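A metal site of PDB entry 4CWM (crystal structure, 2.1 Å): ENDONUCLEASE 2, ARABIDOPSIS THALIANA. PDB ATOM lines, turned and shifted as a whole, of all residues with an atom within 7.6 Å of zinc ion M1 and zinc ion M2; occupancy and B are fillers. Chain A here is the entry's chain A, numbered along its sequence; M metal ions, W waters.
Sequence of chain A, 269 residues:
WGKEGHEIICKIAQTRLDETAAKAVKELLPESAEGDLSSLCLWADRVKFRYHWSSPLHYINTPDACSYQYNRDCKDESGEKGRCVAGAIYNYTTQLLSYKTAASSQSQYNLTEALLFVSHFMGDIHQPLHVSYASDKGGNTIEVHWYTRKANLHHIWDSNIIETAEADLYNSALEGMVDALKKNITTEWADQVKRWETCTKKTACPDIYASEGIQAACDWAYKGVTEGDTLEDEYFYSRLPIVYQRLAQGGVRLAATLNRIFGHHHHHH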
ATOM      1  N   TRP A   1      30.614 -24.806 -28.306  1.00  0.00           N
ATOM      2  CA  TRP A   1      31.926 -25.500 -28.415  1.00  0.00           C
ATOM      3  C   TRP A   1      32.067 -26.625 -27.422  1.00  0.00           C
ATOM      4  O   TRP A   1      31.364 -26.693 -26.416  1.00  0.00           O
ATOM      5  CB  TRP A   1      33.096 -24.552 -28.135  1.00  0.00           C
ATOM      6  CG  TRP A   1      33.040 -23.251 -28.846  1.00  0.00           C
ATOM      7  CD1 TRP A   1      32.466 -22.104 -28.395  1.00  0.00           C
ATOM      8  CD2 TRP A   1      33.613 -22.954 -30.116  1.00  0.00           C
ATOM      9  NE1 TRP A   1      32.646 -21.103 -29.310  1.00  0.00           N
ATOM     10  CE2 TRP A   1      33.355 -21.608 -30.384  1.00  0.00           C
ATOM     11  CE3 TRP A   1      34.327 -23.691 -31.056  1.00  0.00           C
ATOM     12  CZ2 TRP A   1      33.770 -20.974 -31.547  1.00  0.00           C
ATOM     13  CZ3 TRP A   1      34.757 -23.074 -32.227  1.00  0.00           C
ATOM     14  CH2 TRP A   1      34.467 -21.732 -32.457  1.00  0.00           C
ATOM     15  N   GLY A   2      33.017 -27.491 -27.686  1.00  0.00           N
ATOM     16  CA  GLY A   2      33.371 -28.500 -26.736  1.00  0.00           C
ATOM     17  C   GLY A   2      34.264 -27.832 -25.717  1.00  0.00           C
ATOM     18  O   GLY A   2      34.384 -26.603 -25.671  1.00  0.00           O
ATOM     19  N   LYS A   3      34.925 -28.657 -24.941  1.00  0.00           N
ATOM     20  CA  LYS A   3      35.663 -28.203 -23.773  1.00  0.00           C
ATOM     21  C   LYS A   3      36.809 -27.264 -24.069  1.00  0.00           C
ATOM     22  O   LYS A   3      36.940 -26.241 -23.398  1.00  0.00           O
ATOM     23  CB  LYS A   3      36.171 -29.425 -23.003  1.00  0.00           C
ATOM     24  CG  LYS A   3      36.988 -29.061 -21.780  1.00  0.00           C
ATOM     25  CD  LYS A   3      38.470 -29.356 -21.993  1.00  0.00           C
ATOM     26  CE  LYS A   3      38.943 -30.502 -21.122  1.00  0.00           C
ATOM     27  NZ  LYS A   3      39.199 -30.020 -19.735  1.00  0.00           N
ATOM     28  N   GLY A   5      37.331 -25.269 -26.661  1.00  0.00           N
ATOM     29  CA  GLY A   5      36.889 -23.958 -27.142  1.00  0.00           C
ATOM     30  C   GLY A   5      36.459 -23.081 -25.989  1.00  0.00           C
ATOM     31  O   GLY A   5      36.860 -21.918 -25.904  1.00  0.00           O
ATOM     32  N   HIS A   6      35.666 -23.624 -25.077  1.00  0.00           N
ATOM     33  CA  HIS A   6      35.208 -22.845 -23.918  1.00  0.00           C
ATOM     34  C   HIS A   6      36.345 -22.458 -22.963  1.00  0.00           C
ATOM     35  O   HIS A   6      36.332 -21.372 -22.360  1.00  0.00           O
ATOM     36  CB  HIS A   6      34.109 -23.619 -23.160  1.00  0.00           C
ATOM     37  CG  HIS A   6      32.777 -23.598 -23.857  1.00  0.00           C
ATOM     38  ND1 HIS A   6      32.033 -22.452 -23.995  1.00  0.00           N
ATOM     39  CD2 HIS A   6      32.077 -24.579 -24.468  1.00  0.00           C
ATOM     40  CE1 HIS A   6      30.913 -22.728 -24.646  1.00  0.00           C
ATOM     41  NE2 HIS A   6      30.922 -24.008 -24.939  1.00  0.00           N
ATOM     42  N   CYS A  41      33.566 -23.325 -17.227  1.00  0.00           N
ATOM     43  CA  CYS A  41      32.929 -22.757 -18.410  1.00  0.00           C
ATOM     44  C   CYS A  41      32.242 -23.815 -19.275  1.00  0.00           C
ATOM     45  O   CYS A  41      31.615 -23.472 -20.276  1.00  0.00           O
ATOM     46  CB  CYS A  41      33.881 -21.868 -19.221  1.00  0.00           C
ATOM     47  SG  CYS A  41      34.185 -20.240 -18.481  1.00  0.00           S
ATOM     48  N   LEU A  42      32.331 -25.083 -18.898  1.00  0.00           N
ATOM     49  CA  LEU A  42      31.528 -26.143 -19.540  1.00  0.00           C
ATOM     50  C   LEU A  42      30.357 -26.551 -18.682  1.00  0.00           C
ATOM     51  O   LEU A  42      29.555 -27.360 -19.116  1.00  0.00           O
ATOM     52  CB  LEU A  42      32.372 -27.372 -19.890  1.00  0.00           C
ATOM     53  CG  LEU A  42      31.992 -28.147 -21.149  1.00  0.00           C
ATOM     54  CD1 LEU A  42      32.181 -27.342 -22.448  1.00  0.00           C
ATOM     55  CD2 LEU A  42      32.826 -29.407 -21.195  1.00  0.00           C
ATOM     56  N   ALA A  44      27.490 -25.306 -17.956  1.00  0.00           N
ATOM     57  CA  ALA A  44      26.186 -25.241 -18.594  1.00  0.00           C
ATOM     58  C   ALA A  44      25.874 -26.493 -19.460  1.00  0.00           C
ATOM     59  O   ALA A  44      24.719 -26.885 -19.600  1.00  0.00           O
ATOM     60  CB  ALA A  44      26.097 -23.984 -19.434  1.00  0.00           C
ATOM     61  N   ASP A  45      26.893 -27.139 -20.021  1.00  0.00           N
ATOM     62  CA  ASP A  45      26.623 -28.308 -20.882  1.00  0.00           C
ATOM     63  C   ASP A  45      26.199 -29.527 -20.037  1.00  0.00           C
ATOM     64  O   ASP A  45      25.655 -30.494 -20.566  1.00  0.00           O
ATOM     65  CB  ASP A  45      27.819 -28.661 -21.768  1.00  0.00           C
ATOM     66  CG  ASP A  45      27.865 -27.860 -23.089  1.00  0.00           C
ATOM     67  OD1 ASP A  45      26.824 -27.369 -23.593  1.00  0.00           O
ATOM     68  OD2 ASP A  45      28.983 -27.748 -23.631  1.00  0.00           O
ATOM     69  N   ARG A  46      26.467 -29.474 -18.730  1.00  0.00           N
ATOM     70  CA  ARG A  46      26.175 -30.572 -17.805  1.00  0.00           C
ATOM     71  C   ARG A  46      24.800 -30.444 -17.185  1.00  0.00           C
ATOM     72  O   ARG A  46      24.360 -31.369 -16.531  1.00  0.00           O
ATOM     73  CB  ARG A  46      27.205 -30.611 -16.659  1.00  0.00           C
ATOM     74  CG  ARG A  46      28.635 -30.801 -17.117  1.00  0.00           C
ATOM     75  CD  ARG A  46      29.618 -30.902 -15.959  1.00  0.00           C
ATOM     76  NE  ARG A  46      30.196 -29.618 -15.527  1.00  0.00           N
ATOM     77  CZ  ARG A  46      31.382 -29.141 -15.897  1.00  0.00           C
ATOM     78  NH1 ARG A  46      32.169 -29.820 -16.736  1.00  0.00           N
ATOM     79  NH2 ARG A  46      31.798 -27.970 -15.407  1.00  0.00           N
ATOM     80  N   LYS A  48      21.812 -29.556 -19.026  1.00  0.00           N
ATOM     81  CA  LYS A  48      20.733 -29.522 -20.025  1.00  0.00           C
ATOM     82  C   LYS A  48      19.472 -30.336 -19.661  1.00  0.00           C
ATOM     83  O   LYS A  48      18.400 -30.034 -20.130  1.00  0.00           O
ATOM     84  CB  LYS A  48      21.224 -29.988 -21.403  1.00  0.00           C
ATOM     85  CG  LYS A  48      22.346 -29.137 -21.984  1.00  0.00           C
ATOM     86  CD  LYS A  48      22.638 -29.530 -23.415  1.00  0.00           C
ATOM     87  CE  LYS A  48      23.711 -28.683 -24.020  1.00  0.00           C
ATOM     88  NZ  LYS A  48      24.141 -29.307 -25.307  1.00  0.00           N
ATOM     89  N   SER A  55      18.172 -26.039 -22.315  1.00  0.00           N
ATOM     90  CA  SER A  55      18.838 -26.655 -23.452  1.00  0.00           C
ATOM     91  C   SER A  55      18.699 -25.896 -24.774  1.00  0.00           C
ATOM     92  O   SER A  55      19.655 -25.860 -25.565  1.00  0.00           O
ATOM     93  CB  SER A  55      18.535 -28.174 -23.598  1.00  0.00           C
ATOM     94  OG  SER A  55      17.191 -28.463 -23.903  1.00  0.00           O
ATOM     95  N   LEU A  57      18.913 -22.847 -24.980  1.00  0.00           N
ATOM     96  CA  LEU A  57      19.603 -21.607 -24.707  1.00  0.00           C
ATOM     97  C   LEU A  57      21.025 -21.659 -25.209  1.00  0.00           C
ATOM     98  O   LEU A  57      21.734 -20.665 -25.143  1.00  0.00           O
ATOM     99  CB  LEU A  57      19.625 -21.299 -23.202  1.00  0.00           C
ATOM    100  CG  LEU A  57      18.260 -21.233 -22.504  1.00  0.00           C
ATOM    101  CD1 LEU A  57      18.354 -20.962 -21.020  1.00  0.00           C
ATOM    102  CD2 LEU A  57      17.365 -20.180 -23.170  1.00  0.00           C
ATOM    103  N   HIS A  58      21.431 -22.828 -25.691  1.00  0.00           N
ATOM    104  CA  HIS A  58      22.789 -23.007 -26.177  1.00  0.00           C
ATOM    105  C   HIS A  58      22.969 -22.605 -27.651  1.00  0.00           C
ATOM    106  O   HIS A  58      24.083 -22.538 -28.120  1.00  0.00           O
ATOM    107  CB  HIS A  58      23.215 -24.436 -25.989  1.00  0.00           C
ATOM    108  CG  HIS A  58      23.413 -24.818 -24.556  1.00  0.00           C
ATOM    109  ND1 HIS A  58      24.645 -25.034 -24.011  1.00  0.00           N
ATOM    110  CD2 HIS A  58      22.523 -25.012 -23.553  1.00  0.00           C
ATOM    111  CE1 HIS A  58      24.525 -25.340 -22.723  1.00  0.00           C
ATOM    112  NE2 HIS A  58      23.240 -25.331 -22.427  1.00  0.00           N
ATOM    113  N   TYR A  59      21.882 -22.346 -28.380  1.00  0.00           N
ATOM    114  CA  TYR A  59      21.971 -22.170 -29.850  1.00  0.00           C
ATOM    115  C   TYR A  59      20.847 -21.313 -30.406  1.00  0.00           C
ATOM    116  O   TYR A  59      19.983 -20.890 -29.670  1.00  0.00           O
ATOM    117  CB  TYR A  59      21.956 -23.543 -30.560  1.00  0.00           C
ATOM    118  CG  TYR A  59      20.722 -24.341 -30.204  1.00  0.00           C
ATOM    119  CD1 TYR A  59      19.510 -24.170 -30.905  1.00  0.00           C
ATOM    120  CD2 TYR A  59      20.738 -25.216 -29.113  1.00  0.00           C
ATOM    121  CE1 TYR A  59      18.376 -24.906 -30.567  1.00  0.00           C
ATOM    122  CE2 TYR A  59      19.613 -25.949 -28.765  1.00  0.00           C
ATOM    123  CZ  TYR A  59      18.434 -25.782 -29.482  1.00  0.00           C
ATOM    124  OH  TYR A  59      17.345 -26.510 -29.071  1.00  0.00           O
ATOM    125  N   VAL A  85      20.207 -18.692 -27.448  1.00  0.00           N
ATOM    126  CA  VAL A  85      21.474 -18.227 -26.883  1.00  0.00           C
ATOM    127  C   VAL A  85      21.551 -16.700 -26.767  1.00  0.00           C
ATOM    128  O   VAL A  85      22.063 -16.196 -25.795  1.00  0.00           O
ATOM    129  CB  VAL A  85      22.710 -18.839 -27.591  1.00  0.00           C
ATOM    130  CG1 VAL A  85      22.901 -18.241 -28.991  1.00  0.00           C
ATOM    131  CG2 VAL A  85      23.931 -18.602 -26.756  1.00  0.00           C
ATOM    132  N   HIS A 120      29.410 -19.345 -20.581  1.00  0.00           N
ATOM    133  CA  HIS A 120      29.218 -20.425 -21.544  1.00  0.00           C
ATOM    134  C   HIS A 120      28.530 -19.971 -22.813  1.00  0.00           C
ATOM    135  O   HIS A 120      28.950 -20.297 -23.906  1.00  0.00           O
ATOM    136  CB  HIS A 120      28.404 -21.508 -20.906  1.00  0.00           C
ATOM    137  CG  HIS A 120      28.275 -22.708 -21.772  1.00  0.00           C
ATOM    138  ND1 HIS A 120      29.247 -23.672 -21.854  1.00  0.00           N
ATOM    139  CD2 HIS A 120      27.293 -23.087 -22.604  1.00  0.00           C
ATOM    140  CE1 HIS A 120      28.859 -24.608 -22.695  1.00  0.00           C
ATOM    141  NE2 HIS A 120      27.686 -24.259 -23.187  1.00  0.00           N
ATOM    142  N   PHE A 121      27.451 -19.187 -22.652  1.00  0.00           N
ATOM    143  CA  PHE A 121      26.671 -18.769 -23.783  1.00  0.00           C
ATOM    144  C   PHE A 121      27.402 -17.754 -24.674  1.00  0.00           C
ATOM    145  O   PHE A 121      27.239 -17.794 -25.903  1.00  0.00           O
ATOM    146  CB  PHE A 121      25.310 -18.264 -23.318  1.00  0.00           C
ATOM    147  CG  PHE A 121      24.459 -19.331 -22.644  1.00  0.00           C
ATOM    148  CD1 PHE A 121      24.542 -20.677 -23.035  1.00  0.00           C
ATOM    149  CD2 PHE A 121      23.577 -18.994 -21.619  1.00  0.00           C
ATOM    150  CE1 PHE A 121      23.781 -21.635 -22.404  1.00  0.00           C
ATOM    151  CE2 PHE A 121      22.797 -19.949 -21.010  1.00  0.00           C
ATOM    152  CZ  PHE A 121      22.897 -21.281 -21.402  1.00  0.00           C
ATOM    153  N   GLY A 123      30.490 -17.911 -25.261  1.00  0.00           N
ATOM    154  CA  GLY A 123      31.256 -18.818 -26.081  1.00  0.00           C
ATOM    155  C   GLY A 123      30.429 -19.481 -27.186  1.00  0.00           C
ATOM    156  O   GLY A 123      30.852 -19.494 -28.339  1.00  0.00           O
ATOM    157  N   ASP A 124      29.276 -20.012 -26.818  1.00  0.00           N
ATOM    158  CA  ASP A 124      28.402 -20.731 -27.771  1.00  0.00           C
ATOM    159  C   ASP A 124      27.879 -19.847 -28.854  1.00  0.00           C
ATOM    160  O   ASP A 124      27.839 -20.310 -29.962  1.00  0.00           O
ATOM    161  CB  ASP A 124      27.217 -21.422 -27.109  1.00  0.00           C
ATOM    162  CG  ASP A 124      27.530 -22.828 -26.669  1.00  0.00           C
ATOM    163  OD1 ASP A 124      28.658 -23.257 -26.808  1.00  0.00           O
ATOM    164  OD2 ASP A 124      26.645 -23.487 -26.147  1.00  0.00           O
ATOM    165  N   ILE A 125      27.495 -18.591 -28.559  1.00  0.00           N
ATOM    166  CA  ILE A 125      26.994 -17.677 -29.603  1.00  0.00           C
ATOM    167  C   ILE A 125      28.035 -17.364 -30.675  1.00  0.00           C
ATOM    168  O   ILE A 125      27.725 -16.855 -31.766  1.00  0.00           O
ATOM    169  CB  ILE A 125      26.384 -16.368 -29.019  1.00  0.00           C
ATOM    170  CG1 ILE A 125      25.370 -15.781 -30.004  1.00  0.00           C
ATOM    171  CG2 ILE A 125      27.471 -15.341 -28.693  1.00  0.00           C
ATOM    172  CD1 ILE A 125      24.409 -14.728 -29.426  1.00  0.00           C
ATOM    173  N   GLN A 127      30.202 -19.872 -31.773  1.00  0.00           N
ATOM    174  CA  GLN A 127      30.278 -21.073 -32.612  1.00  0.00           C
ATOM    175  C   GLN A 127      29.350 -20.884 -33.825  1.00  0.00           C
ATOM    176  O   GLN A 127      28.133 -20.740 -33.657  1.00  0.00           O
ATOM    177  CB  GLN A 127      29.889 -22.342 -31.821  1.00  0.00           C
ATOM    178  CG  GLN A 127      30.739 -23.599 -32.147  1.00  0.00           C
ATOM    179  CD  GLN A 127      30.359 -24.274 -33.446  1.00  0.00           C
ATOM    180  OE1 GLN A 127      30.355 -23.673 -34.520  1.00  0.00           O
ATOM    181  NE2 GLN A 127      30.068 -25.559 -33.360  1.00  0.00           N
ATOM    182  N   HIS A 130      26.329 -22.985 -33.909  1.00  0.00           N
ATOM    183  CA  HIS A 130      25.316 -22.805 -32.830  1.00  0.00           C
ATOM    184  C   HIS A 130      24.321 -21.712 -33.206  1.00  0.00           C
ATOM    185  O   HIS A 130      23.420 -21.372 -32.395  1.00  0.00           O
ATOM    186  CB  HIS A 130      25.964 -22.447 -31.500  1.00  0.00           C
ATOM    187  CG  HIS A 130      26.378 -23.626 -30.711  1.00  0.00           C
ATOM    188  ND1 HIS A 130      25.755 -23.989 -29.549  1.00  0.00           N
ATOM    189  CD2 HIS A 130      27.298 -24.589 -30.958  1.00  0.00           C
ATOM    190  CE1 HIS A 130      26.274 -25.131 -29.108  1.00  0.00           C
ATOM    191  NE2 HIS A 130      27.233 -25.500 -29.931  1.00  0.00           N
ATOM    192  N   HIS A 154      28.760 -30.492 -37.160  1.00  0.00           N
ATOM    193  CA  HIS A 154      28.647 -29.654 -35.987  1.00  0.00           C
ATOM    194  C   HIS A 154      29.822 -29.944 -35.077  1.00  0.00           C
ATOM    195  O   HIS A 154      30.473 -29.029 -34.585  1.00  0.00           O
ATOM    196  CB  HIS A 154      27.340 -29.939 -35.232  1.00  0.00           C
ATOM    197  CG  HIS A 154      27.137 -29.069 -34.050  1.00  0.00           C
ATOM    198  ND1 HIS A 154      26.524 -27.836 -34.145  1.00  0.00           N
ATOM    199  CD2 HIS A 154      27.504 -29.213 -32.767  1.00  0.00           C
ATOM    200  CE1 HIS A 154      26.542 -27.256 -32.959  1.00  0.00           C
ATOM    201  NE2 HIS A 154      27.144 -28.065 -32.108  1.00  0.00           N
ATOM    202  N   ASP A 158      32.680 -27.757 -33.151  1.00  0.00           N
ATOM    203  CA  ASP A 158      32.783 -27.743 -31.672  1.00  0.00           C
ATOM    204  C   ASP A 158      34.172 -28.093 -31.172  1.00  0.00           C
ATOM    205  O   ASP A 158      34.692 -27.421 -30.285  1.00  0.00           O
ATOM    206  CB  ASP A 158      31.804 -28.732 -31.046  1.00  0.00           C
ATOM    207  CG  ASP A 158      30.432 -28.155 -30.841  1.00  0.00           C
ATOM    208  OD1 ASP A 158      30.287 -26.934 -30.976  1.00  0.00           O
ATOM    209  OD2 ASP A 158      29.490 -28.919 -30.504  1.00  0.00           O
HETATM  210 ZN    ZN M   1      26.670 -25.434 -24.976  1.00  0.00          ZN
HETATM  211 ZN    ZN M   2      29.796 -25.015 -26.389  1.00  0.00          ZN
HETATM  212 ZN    ZN M   3      27.853 -27.546 -30.203  1.00  0.00          ZN
HETATM  213  O   HOH W   1      28.447 -27.491 -28.164  1.00  0.00           O
HETATM  214  O   HOH W   2      28.378 -26.343 -25.878  1.00  0.00           O
HETATM  215  O   HOH W   3      25.475 -26.940 -26.415  1.00  0.00           O
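ND1 of His 120 lies within hydrogen-bond range of O of Cys 41, 2.9 Å away. The backbone NH (N) of Trp 1 sits close to the side-chain carboxylate (OD1) of Asp 158, 3.4 Å away. The indole nitrogen (NE1) of Trp 1 lies within hydrogen-bond range of the backbone carbonyl oxygen (O) of Gly 123, at 2.6 Å. The backbone carbonyl oxygen (O) of His 58 lies within hydrogen-bond range of a ring nitrogen (ND1) of His 130. OD1 of Asp 45 lies close to NZ of Lys 48 (3.7 Å).
Within 4 Å of zinc ion M2: Trp 1, His 6, Asp 45, His 120 and Asp 124.
Zinc ion M1 is bound by water W2 (2.1 Å), the side-chain carboxylate (OD2) of Asp 124 (2.3 Å), a ring nitrogen (ND1) of His 58 (2.3 Å), a ring nitrogen (NE2) of His 120 (2.4 Å), the side-chain carboxylate (OD1) of Asp 45 (2.4 Å) and water W3 (2.4 Å).
Of the 25 residues printed, 4 come within 4 Å of zinc ion M1. The nearest printed residue that does not touch zinc ion M1 is His 130 (4.2 Å).
Zinc ion M2 is bound by water W2 (2.0 Å), NE2 of His 6 (2.1 Å), N of Trp 1 (2.1 Å), OD1 of Asp 124 (2.1 Å) and O of Trp 1 (2.3 Å). Zinc ion M2 has five donor atoms within binding distance.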
